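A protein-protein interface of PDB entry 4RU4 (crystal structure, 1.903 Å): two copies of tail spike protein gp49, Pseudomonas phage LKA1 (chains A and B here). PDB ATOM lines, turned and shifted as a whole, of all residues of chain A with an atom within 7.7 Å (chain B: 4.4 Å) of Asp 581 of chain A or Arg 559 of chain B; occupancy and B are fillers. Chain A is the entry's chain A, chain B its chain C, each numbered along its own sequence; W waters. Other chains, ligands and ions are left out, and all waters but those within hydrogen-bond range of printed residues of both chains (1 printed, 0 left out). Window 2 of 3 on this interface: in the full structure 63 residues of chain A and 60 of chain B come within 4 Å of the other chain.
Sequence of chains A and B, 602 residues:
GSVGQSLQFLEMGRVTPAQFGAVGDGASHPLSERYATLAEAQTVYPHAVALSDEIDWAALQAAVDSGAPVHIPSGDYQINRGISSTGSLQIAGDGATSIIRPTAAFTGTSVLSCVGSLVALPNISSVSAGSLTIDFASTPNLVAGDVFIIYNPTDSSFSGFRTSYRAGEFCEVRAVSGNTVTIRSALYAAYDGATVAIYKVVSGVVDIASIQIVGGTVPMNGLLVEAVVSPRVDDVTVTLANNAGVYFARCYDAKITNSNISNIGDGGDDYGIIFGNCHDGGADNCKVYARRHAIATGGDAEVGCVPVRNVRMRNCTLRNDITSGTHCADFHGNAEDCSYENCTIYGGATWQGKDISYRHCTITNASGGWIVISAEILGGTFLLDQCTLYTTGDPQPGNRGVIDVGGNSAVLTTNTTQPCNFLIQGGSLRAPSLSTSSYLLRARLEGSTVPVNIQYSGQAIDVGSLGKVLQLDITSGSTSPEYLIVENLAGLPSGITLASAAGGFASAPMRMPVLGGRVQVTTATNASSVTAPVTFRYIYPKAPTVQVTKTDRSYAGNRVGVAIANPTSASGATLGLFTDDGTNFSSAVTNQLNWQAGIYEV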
ATOM      1  N   SER A 528     -13.566  28.488 -25.993  1.00  0.00           N
ATOM      2  CA  SER A 528     -12.776  27.536 -26.777  1.00  0.00           C
ATOM      3  C   SER A 528     -13.481  26.185 -26.906  1.00  0.00           C
ATOM      4  O   SER A 528     -12.908  25.229 -27.436  1.00  0.00           O
ATOM      5  CB  SER A 528     -11.403  27.317 -26.140  1.00  0.00           C
ATOM      6  OG  SER A 528     -11.515  26.590 -24.924  1.00  0.00           O
ATOM      7  N   ASN A 558     -11.491  29.817 -36.969  1.00  0.00           N
ATOM      8  CA  ASN A 558     -10.026  29.738 -36.821  1.00  0.00           C
ATOM      9  C   ASN A 558      -9.496  28.368 -36.383  1.00  0.00           C
ATOM     10  O   ASN A 558      -8.278  28.146 -36.332  1.00  0.00           O
ATOM     11  CB  ASN A 558      -9.561  30.798 -35.802  1.00  0.00           C
ATOM     12  CG  ASN A 558     -10.209  30.611 -34.430  1.00  0.00           C
ATOM     13  OD1 ASN A 558     -11.231  29.904 -34.297  1.00  0.00           O
ATOM     14  ND2 ASN A 558      -9.641  31.264 -33.405  1.00  0.00           N
ATOM     15  N   ARG A 559     -10.406  27.464 -36.035  1.00  0.00           N
ATOM     16  CA  ARG A 559     -10.025  26.170 -35.442  1.00  0.00           C
ATOM     17  C   ARG A 559     -10.992  25.083 -35.916  1.00  0.00           C
ATOM     18  O   ARG A 559     -12.189  25.332 -36.109  1.00  0.00           O
ATOM     19  CB  ARG A 559     -10.079  26.226 -33.896  1.00  0.00           C
ATOM     20  CG  ARG A 559      -9.011  27.115 -33.223  1.00  0.00           C
ATOM     21  CD  ARG A 559      -7.659  26.460 -33.389  1.00  0.00           C
ATOM     22  NE  ARG A 559      -6.576  27.235 -32.799  1.00  0.00           N
ATOM     23  CZ  ARG A 559      -6.032  28.342 -33.310  1.00  0.00           C
ATOM     24  NH1 ARG A 559      -6.436  28.855 -34.466  1.00  0.00           N
ATOM     25  NH2 ARG A 559      -5.030  28.923 -32.661  1.00  0.00           N
ATOM     26  N   VAL A 562     -11.373  19.694 -31.432  1.00  0.00           N
ATOM     27  CA  VAL A 562     -11.146  18.283 -31.152  1.00  0.00           C
ATOM     28  C   VAL A 562     -12.374  17.733 -30.461  1.00  0.00           C
ATOM     29  O   VAL A 562     -12.795  18.240 -29.411  1.00  0.00           O
ATOM     30  CB  VAL A 562      -9.917  18.084 -30.232  1.00  0.00           C
ATOM     31  CG1 VAL A 562      -9.644  16.583 -30.012  1.00  0.00           C
ATOM     32  CG2 VAL A 562      -8.705  18.741 -30.855  1.00  0.00           C
ATOM     33  N   PHE A 578     -13.532  20.997 -28.594  1.00  0.00           N
ATOM     34  CA  PHE A 578     -12.581  21.889 -27.911  1.00  0.00           C
ATOM     35  C   PHE A 578     -11.423  22.271 -28.850  1.00  0.00           C
ATOM     36  O   PHE A 578     -10.812  21.403 -29.451  1.00  0.00           O
ATOM     37  CB  PHE A 578     -11.970  21.187 -26.691  1.00  0.00           C
ATOM     38  CG  PHE A 578     -12.918  20.998 -25.530  1.00  0.00           C
ATOM     39  CD1 PHE A 578     -13.973  20.110 -25.614  1.00  0.00           C
ATOM     40  CD2 PHE A 578     -12.700  21.664 -24.332  1.00  0.00           C
ATOM     41  CE1 PHE A 578     -14.839  19.924 -24.529  1.00  0.00           C
ATOM     42  CE2 PHE A 578     -13.555  21.492 -23.258  1.00  0.00           C
ATOM     43  CZ  PHE A 578     -14.626  20.627 -23.355  1.00  0.00           C
ATOM     44  N   THR A 579     -11.095  23.549 -28.963  1.00  0.00           N
ATOM     45  CA  THR A 579      -9.890  23.905 -29.709  1.00  0.00           C
ATOM     46  C   THR A 579      -8.693  23.292 -28.982  1.00  0.00           C
ATOM     47  O   THR A 579      -8.651  23.261 -27.738  1.00  0.00           O
ATOM     48  CB  THR A 579      -9.728  25.441 -29.904  1.00  0.00           C
ATOM     49  OG1 THR A 579      -9.336  26.045 -28.665  1.00  0.00           O
ATOM     50  CG2 THR A 579     -11.048  26.068 -30.394  1.00  0.00           C
ATOM     51  N   ASP A 580      -7.725  22.789 -29.741  1.00  0.00           N
ATOM     52  CA  ASP A 580      -6.652  22.022 -29.119  1.00  0.00           C
ATOM     53  C   ASP A 580      -5.844  22.893 -28.173  1.00  0.00           C
ATOM     54  O   ASP A 580      -5.460  22.453 -27.085  1.00  0.00           O
ATOM     55  CB  ASP A 580      -5.716  21.371 -30.150  1.00  0.00           C
ATOM     56  CG  ASP A 580      -4.803  20.318 -29.501  1.00  0.00           C
ATOM     57  OD1 ASP A 580      -5.273  19.650 -28.555  1.00  0.00           O
ATOM     58  OD2 ASP A 580      -3.623  20.167 -29.896  1.00  0.00           O
ATOM     59  N   ASP A 581      -5.618  24.139 -28.581  1.00  0.00           N
ATOM     60  CA  ASP A 581      -4.770  25.050 -27.818  1.00  0.00           C
ATOM     61  C   ASP A 581      -5.502  26.038 -26.905  1.00  0.00           C
ATOM     62  O   ASP A 581      -4.862  26.889 -26.283  1.00  0.00           O
ATOM     63  CB  ASP A 581      -3.781  25.794 -28.729  1.00  0.00           C
ATOM     64  CG  ASP A 581      -4.446  26.843 -29.624  1.00  0.00           C
ATOM     65  OD1 ASP A 581      -5.660  27.134 -29.535  1.00  0.00           O
ATOM     66  OD2 ASP A 581      -3.715  27.396 -30.445  1.00  0.00           O
ATOM     67  N   GLY A 582      -6.828  25.941 -26.830  1.00  0.00           N
ATOM     68  CA  GLY A 582      -7.588  26.773 -25.908  1.00  0.00           C
ATOM     69  C   GLY A 582      -7.942  28.151 -26.430  1.00  0.00           C
ATOM     70  O   GLY A 582      -8.570  28.933 -25.720  1.00  0.00           O
ATOM     71  N   THR A 583      -7.519  28.477 -27.656  1.00  0.00           N
ATOM     72  CA  THR A 583      -7.926  29.733 -28.279  1.00  0.00           C
ATOM     73  C   THR A 583      -9.447  29.702 -28.465  1.00  0.00           C
ATOM     74  O   THR A 583      -9.989  28.665 -28.820  1.00  0.00           O
ATOM     75  CB  THR A 583      -7.269  29.882 -29.660  1.00  0.00           C
ATOM     76  OG1 THR A 583      -5.848  29.887 -29.492  1.00  0.00           O
ATOM     77  CG2 THR A 583      -7.697  31.195 -30.330  1.00  0.00           C
ATOM     78  N   ASN A 584     -10.137  30.817 -28.229  1.00  0.00           N
ATOM     79  CA  ASN A 584     -11.571  30.874 -28.521  1.00  0.00           C
ATOM     80  C   ASN A 584     -11.831  30.642 -30.007  1.00  0.00           C
ATOM     81  O   ASN A 584     -11.074  31.108 -30.869  1.00  0.00           O
ATOM     82  CB  ASN A 584     -12.141  32.247 -28.152  1.00  0.00           C
ATOM     83  CG  ASN A 584     -12.243  32.451 -26.672  1.00  0.00           C
ATOM     84  OD1 ASN A 584     -12.209  31.494 -25.891  1.00  0.00           O
ATOM     85  ND2 ASN A 584     -12.389  33.699 -26.264  1.00  0.00           N
ATOM     86  N   SER B 554     -10.680  17.023 -20.269  1.00  0.00           N
ATOM     87  CA  SER B 554     -10.776  18.017 -21.322  1.00  0.00           C
ATOM     88  C   SER B 554      -9.380  18.551 -21.673  1.00  0.00           C
ATOM     89  O   SER B 554      -8.592  17.835 -22.295  1.00  0.00           O
ATOM     90  CB  SER B 554     -11.742  19.121 -20.905  1.00  0.00           C
ATOM     91  OG  SER B 554     -13.071  18.626 -20.977  1.00  0.00           O
ATOM     92  N   TYR B 555      -9.052  19.784 -21.282  1.00  0.00           N
ATOM     93  CA  TYR B 555      -7.660  20.214 -21.389  1.00  0.00           C
ATOM     94  C   TYR B 555      -6.771  19.435 -20.435  1.00  0.00           C
ATOM     95  O   TYR B 555      -7.132  19.245 -19.266  1.00  0.00           O
ATOM     96  CB  TYR B 555      -7.492  21.737 -21.198  1.00  0.00           C
ATOM     97  CG  TYR B 555      -8.094  22.482 -22.378  1.00  0.00           C
ATOM     98  CD1 TYR B 555      -7.441  22.510 -23.608  1.00  0.00           C
ATOM     99  CD2 TYR B 555      -9.357  23.061 -22.286  1.00  0.00           C
ATOM    100  CE1 TYR B 555      -8.004  23.134 -24.698  1.00  0.00           C
ATOM    101  CE2 TYR B 555      -9.936  23.702 -23.382  1.00  0.00           C
ATOM    102  CZ  TYR B 555      -9.261  23.727 -24.583  1.00  0.00           C
ATOM    103  OH  TYR B 555      -9.831  24.340 -25.690  1.00  0.00           O
ATOM    104  N   ALA B 556      -5.635  18.939 -20.947  1.00  0.00           N
ATOM    105  CA  ALA B 556      -4.560  18.439 -20.080  1.00  0.00           C
ATOM    106  C   ALA B 556      -3.569  19.578 -19.884  1.00  0.00           C
ATOM    107  O   ALA B 556      -2.519  19.603 -20.500  1.00  0.00           O
ATOM    108  CB  ALA B 556      -3.858  17.256 -20.699  1.00  0.00           C
ATOM    109  N   GLY B 557      -3.919  20.527 -19.031  1.00  0.00           N
ATOM    110  CA  GLY B 557      -3.167  21.758 -18.927  1.00  0.00           C
ATOM    111  C   GLY B 557      -3.442  22.684 -20.109  1.00  0.00           C
ATOM    112  O   GLY B 557      -4.432  23.412 -20.121  1.00  0.00           O
ATOM    113  N   ASN B 558      -2.549  22.653 -21.095  1.00  0.00           N
ATOM    114  CA  ASN B 558      -2.597  23.565 -22.230  1.00  0.00           C
ATOM    115  C   ASN B 558      -3.191  22.984 -23.510  1.00  0.00           C
ATOM    116  O   ASN B 558      -3.428  23.732 -24.460  1.00  0.00           O
ATOM    117  CB  ASN B 558      -1.177  24.041 -22.552  1.00  0.00           C
ATOM    118  CG  ASN B 558      -0.259  22.901 -22.905  1.00  0.00           C
ATOM    119  OD1 ASN B 558      -0.503  21.766 -22.510  1.00  0.00           O
ATOM    120  ND2 ASN B 558       0.801  23.191 -23.652  1.00  0.00           N
ATOM    121  N   ARG B 559      -3.423  21.666 -23.551  1.00  0.00           N
ATOM    122  CA  ARG B 559      -3.830  21.024 -24.801  1.00  0.00           C
ATOM    123  C   ARG B 559      -4.836  19.902 -24.568  1.00  0.00           C
ATOM    124  O   ARG B 559      -4.798  19.222 -23.539  1.00  0.00           O
ATOM    125  CB  ARG B 559      -2.613  20.426 -25.510  1.00  0.00           C
ATOM    126  CG  ARG B 559      -1.589  21.448 -26.034  1.00  0.00           C
ATOM    127  CD  ARG B 559      -2.100  22.124 -27.295  1.00  0.00           C
ATOM    128  NE  ARG B 559      -1.146  23.055 -27.894  1.00  0.00           N
ATOM    129  CZ  ARG B 559      -0.895  24.285 -27.443  1.00  0.00           C
ATOM    130  NH1 ARG B 559      -1.484  24.742 -26.333  1.00  0.00           N
ATOM    131  NH2 ARG B 559      -0.028  25.054 -28.092  1.00  0.00           N
ATOM    132  N   VAL B 560      -5.733  19.692 -25.528  1.00  0.00           N
ATOM    133  CA  VAL B 560      -6.629  18.525 -25.442  1.00  0.00           C
ATOM    134  C   VAL B 560      -5.880  17.246 -25.848  1.00  0.00           C
ATOM    135  O   VAL B 560      -5.950  16.212 -25.166  1.00  0.00           O
ATOM    136  CB  VAL B 560      -7.858  18.675 -26.375  1.00  0.00           C
ATOM    137  CG1 VAL B 560      -8.735  17.411 -26.279  1.00  0.00           C
ATOM    138  CG2 VAL B 560      -8.667  19.953 -26.027  1.00  0.00           C
ATOM    139  N   GLY B 561      -5.172  17.315 -26.980  1.00  0.00           N
ATOM    140  CA  GLY B 561      -4.489  16.153 -27.517  1.00  0.00           C
ATOM    141  C   GLY B 561      -5.340  15.478 -28.585  1.00  0.00           C
ATOM    142  O   GLY B 561      -6.564  15.353 -28.445  1.00  0.00           O
ATOM    143  N   THR B 579      -0.275  16.359 -28.853  1.00  0.00           N
ATOM    144  CA  THR B 579      -0.741  17.728 -29.055  1.00  0.00           C
ATOM    145  C   THR B 579      -0.611  18.007 -30.540  1.00  0.00           C
ATOM    146  O   THR B 579       0.318  17.504 -31.180  1.00  0.00           O
ATOM    147  CB  THR B 579       0.077  18.729 -28.250  1.00  0.00           C
ATOM    148  OG1 THR B 579       1.408  18.802 -28.784  1.00  0.00           O
ATOM    149  CG2 THR B 579       0.098  18.307 -26.786  1.00  0.00           C
ATOM    150  N   ASP B 581       0.139  20.610 -32.272  1.00  0.00           N
ATOM    151  CA  ASP B 581       1.250  21.468 -32.686  1.00  0.00           C
ATOM    152  C   ASP B 581       2.601  21.026 -32.133  1.00  0.00           C
ATOM    153  O   ASP B 581       3.618  21.664 -32.403  1.00  0.00           O
ATOM    154  CB  ASP B 581       0.977  22.937 -32.314  1.00  0.00           C
ATOM    155  CG  ASP B 581       0.980  23.176 -30.812  1.00  0.00           C
ATOM    156  OD1 ASP B 581       0.907  22.210 -30.032  1.00  0.00           O
ATOM    157  OD2 ASP B 581       1.037  24.342 -30.394  1.00  0.00           O
ATOM    158  N   THR B 583       3.637  21.072 -29.071  1.00  0.00           N
ATOM    159  CA  THR B 583       3.946  21.702 -27.785  1.00  0.00           C
ATOM    160  C   THR B 583       3.849  20.617 -26.710  1.00  0.00           C
ATOM    161  O   THR B 583       2.977  19.749 -26.799  1.00  0.00           O
ATOM    162  CB  THR B 583       2.960  22.866 -27.493  1.00  0.00           C
ATOM    163  OG1 THR B 583       3.127  23.879 -28.489  1.00  0.00           O
ATOM    164  CG2 THR B 583       3.228  23.526 -26.128  1.00  0.00           C
ATOM    165  N   PHE B 585       2.749  18.834 -23.363  1.00  0.00           N
ATOM    166  CA  PHE B 585       1.658  18.980 -22.392  1.00  0.00           C
ATOM    167  C   PHE B 585       2.151  19.724 -21.147  1.00  0.00           C
ATOM    168  O   PHE B 585       3.281  19.543 -20.706  1.00  0.00           O
ATOM    169  CB  PHE B 585       1.121  17.614 -21.979  1.00  0.00           C
ATOM    170  CG  PHE B 585       0.217  16.973 -23.007  1.00  0.00           C
ATOM    171  CD1 PHE B 585      -1.112  17.372 -23.137  1.00  0.00           C
ATOM    172  CD2 PHE B 585       0.688  15.948 -23.813  1.00  0.00           C
ATOM    173  CE1 PHE B 585      -1.973  16.754 -24.081  1.00  0.00           C
ATOM    174  CE2 PHE B 585      -0.145  15.347 -24.756  1.00  0.00           C
ATOM    175  CZ  PHE B 585      -1.473  15.740 -24.889  1.00  0.00           C
HETATM  176  O   HOH W   1      -1.970  22.113 -30.609  1.00  0.00           O
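Asp 581 of chain A touches Asn 558 of chain B, but with the chains exchanged Asn 558 of chain A does not touch Asp 581 of chain B (11.4 Å). Asp 581 of chain A touches Arg 559 of chain B, but with the chains exchanged Arg 559 of chain A does not touch Asp 581 of chain B (7.9 Å). Positions printed for both chains: 558, 559, 579, 581 and 583.
Among the printed residues, merely in contact across the chains: Val 562 of chain A with Val 560 of chain B, Val 562 of chain A with Gly 561 of chain B, Phe 578 of chain A with Ser 554 of chain B, Phe 578 of chain A with Tyr 555 of chain B, Phe 578 of chain A with Val 560 of chain B, Thr 579 of chain A with Val 560 of chain B, Asp 580 of chain A with Tyr 555 of chain B, Asp 580 of chain A with Asn 558 of chain B, Asp 580 of chain A with Arg 559 of chain B, Asp 580 of chain A with Thr 579 of chain B, Asp 581 of chain A with Asn 558 of chain B, Asp 581 of chain A with Arg 559 of chain B and Gly 582 of chain A with Tyr 555 of chain B.
The backbone NH of Thr 579 of chain A is in hydrogen-bond range of the backbone carbonyl oxygen of Ser 528 of chain A (2.9 Å). The backbone NH of Ser 528 of chain A is in hydrogen-bond range of the side-chain amide oxygen of Asn 584 of chain A. NH2 of Arg 559 of chain A lies within salt-bridge range of OD2 of Asp 581 of chain A (3.0 Å). The backbone NH of Val 562 of chain A sits at hydrogen-bond distance from the backbone carbonyl oxygen of Phe 578 of chain A (2.7 Å). The side-chain hydroxyl (OG1) of Thr 579 of chain A lies within hydrogen-bond range of the backbone carbonyl oxygen (O) of Thr 583 of chain A, at 2.7 Å. NH2 of Arg 559 of chain B lies within hydrogen-bond range of OG1 of Thr 583 of chain B, 3.4 Å away.
OG of Ser 528 of chain A lies within hydrogen-bond range of OH of Tyr 555 of chain B. The backbone carbonyl oxygen (O) of Thr 579 of chain A lies within hydrogen-bond range of the side-chain hydroxyl (OH) of Tyr 555 of chain B, at 2.6 Å. The side-chain carboxylate of Asp 580 of chain A lies within hydrogen-bond range of the backbone NH of Val 560 of chain B (3.1 Å). The side-chain carboxylate (OD1) of Asp 580 of chain A sits at hydrogen-bond distance from the backbone NH (N) of Gly 561 of chain B (2.8 Å).
Water W1 lies within hydrogen-bond range of OD2 of Asp 580 of chain A, OD1 of Asp 581 of chain B and NE of Arg 559 of chain B.
Printed residues of chain B within 4 Å of Thr 579 of chain A: Tyr 555 (2.6 Å) and Val 560 (3.7 Å). Asp 581 of chain A touches two residues of chain B. Printed residues of chain B within 4 Å of Gly 582 of chain A: Tyr 555. Ala 556 of chain B touches none of the printed residues of chain A. Printed residues of chain A within 4 Å of Arg 559 of chain B: Asp 580 (3.1 Å) and Asp 581 (3.5 Å). The nearest residue of chain A that does not touch Arg 559 of chain B is Gly 582 of chain A (5.5 Å). The nearest printed residue of chain A that does not touch Thr 579 of chain B is Asp 581 of chain A (7.9 Å).
Hydrophobic or aromatic side chains of chain A within 4 Å of the printed part of chain B: Val 562 and Phe 578. Of the 12 printed residues of chain B, 7 touch a printed residue of chain A. Hydrophobic or aromatic side chains of chain B that line the printed part of chain A: Tyr 555 and Val 560. Along chain B the printed residues that touch a printed residue of chain A span positions 554 to 579. Among the printed residues, 17 pairs touch across the chains. Among the printed residues, no Asp or Glu carboxylate lies within 4 Å of a Lys or Arg side-chain nitrogen of the other chain.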
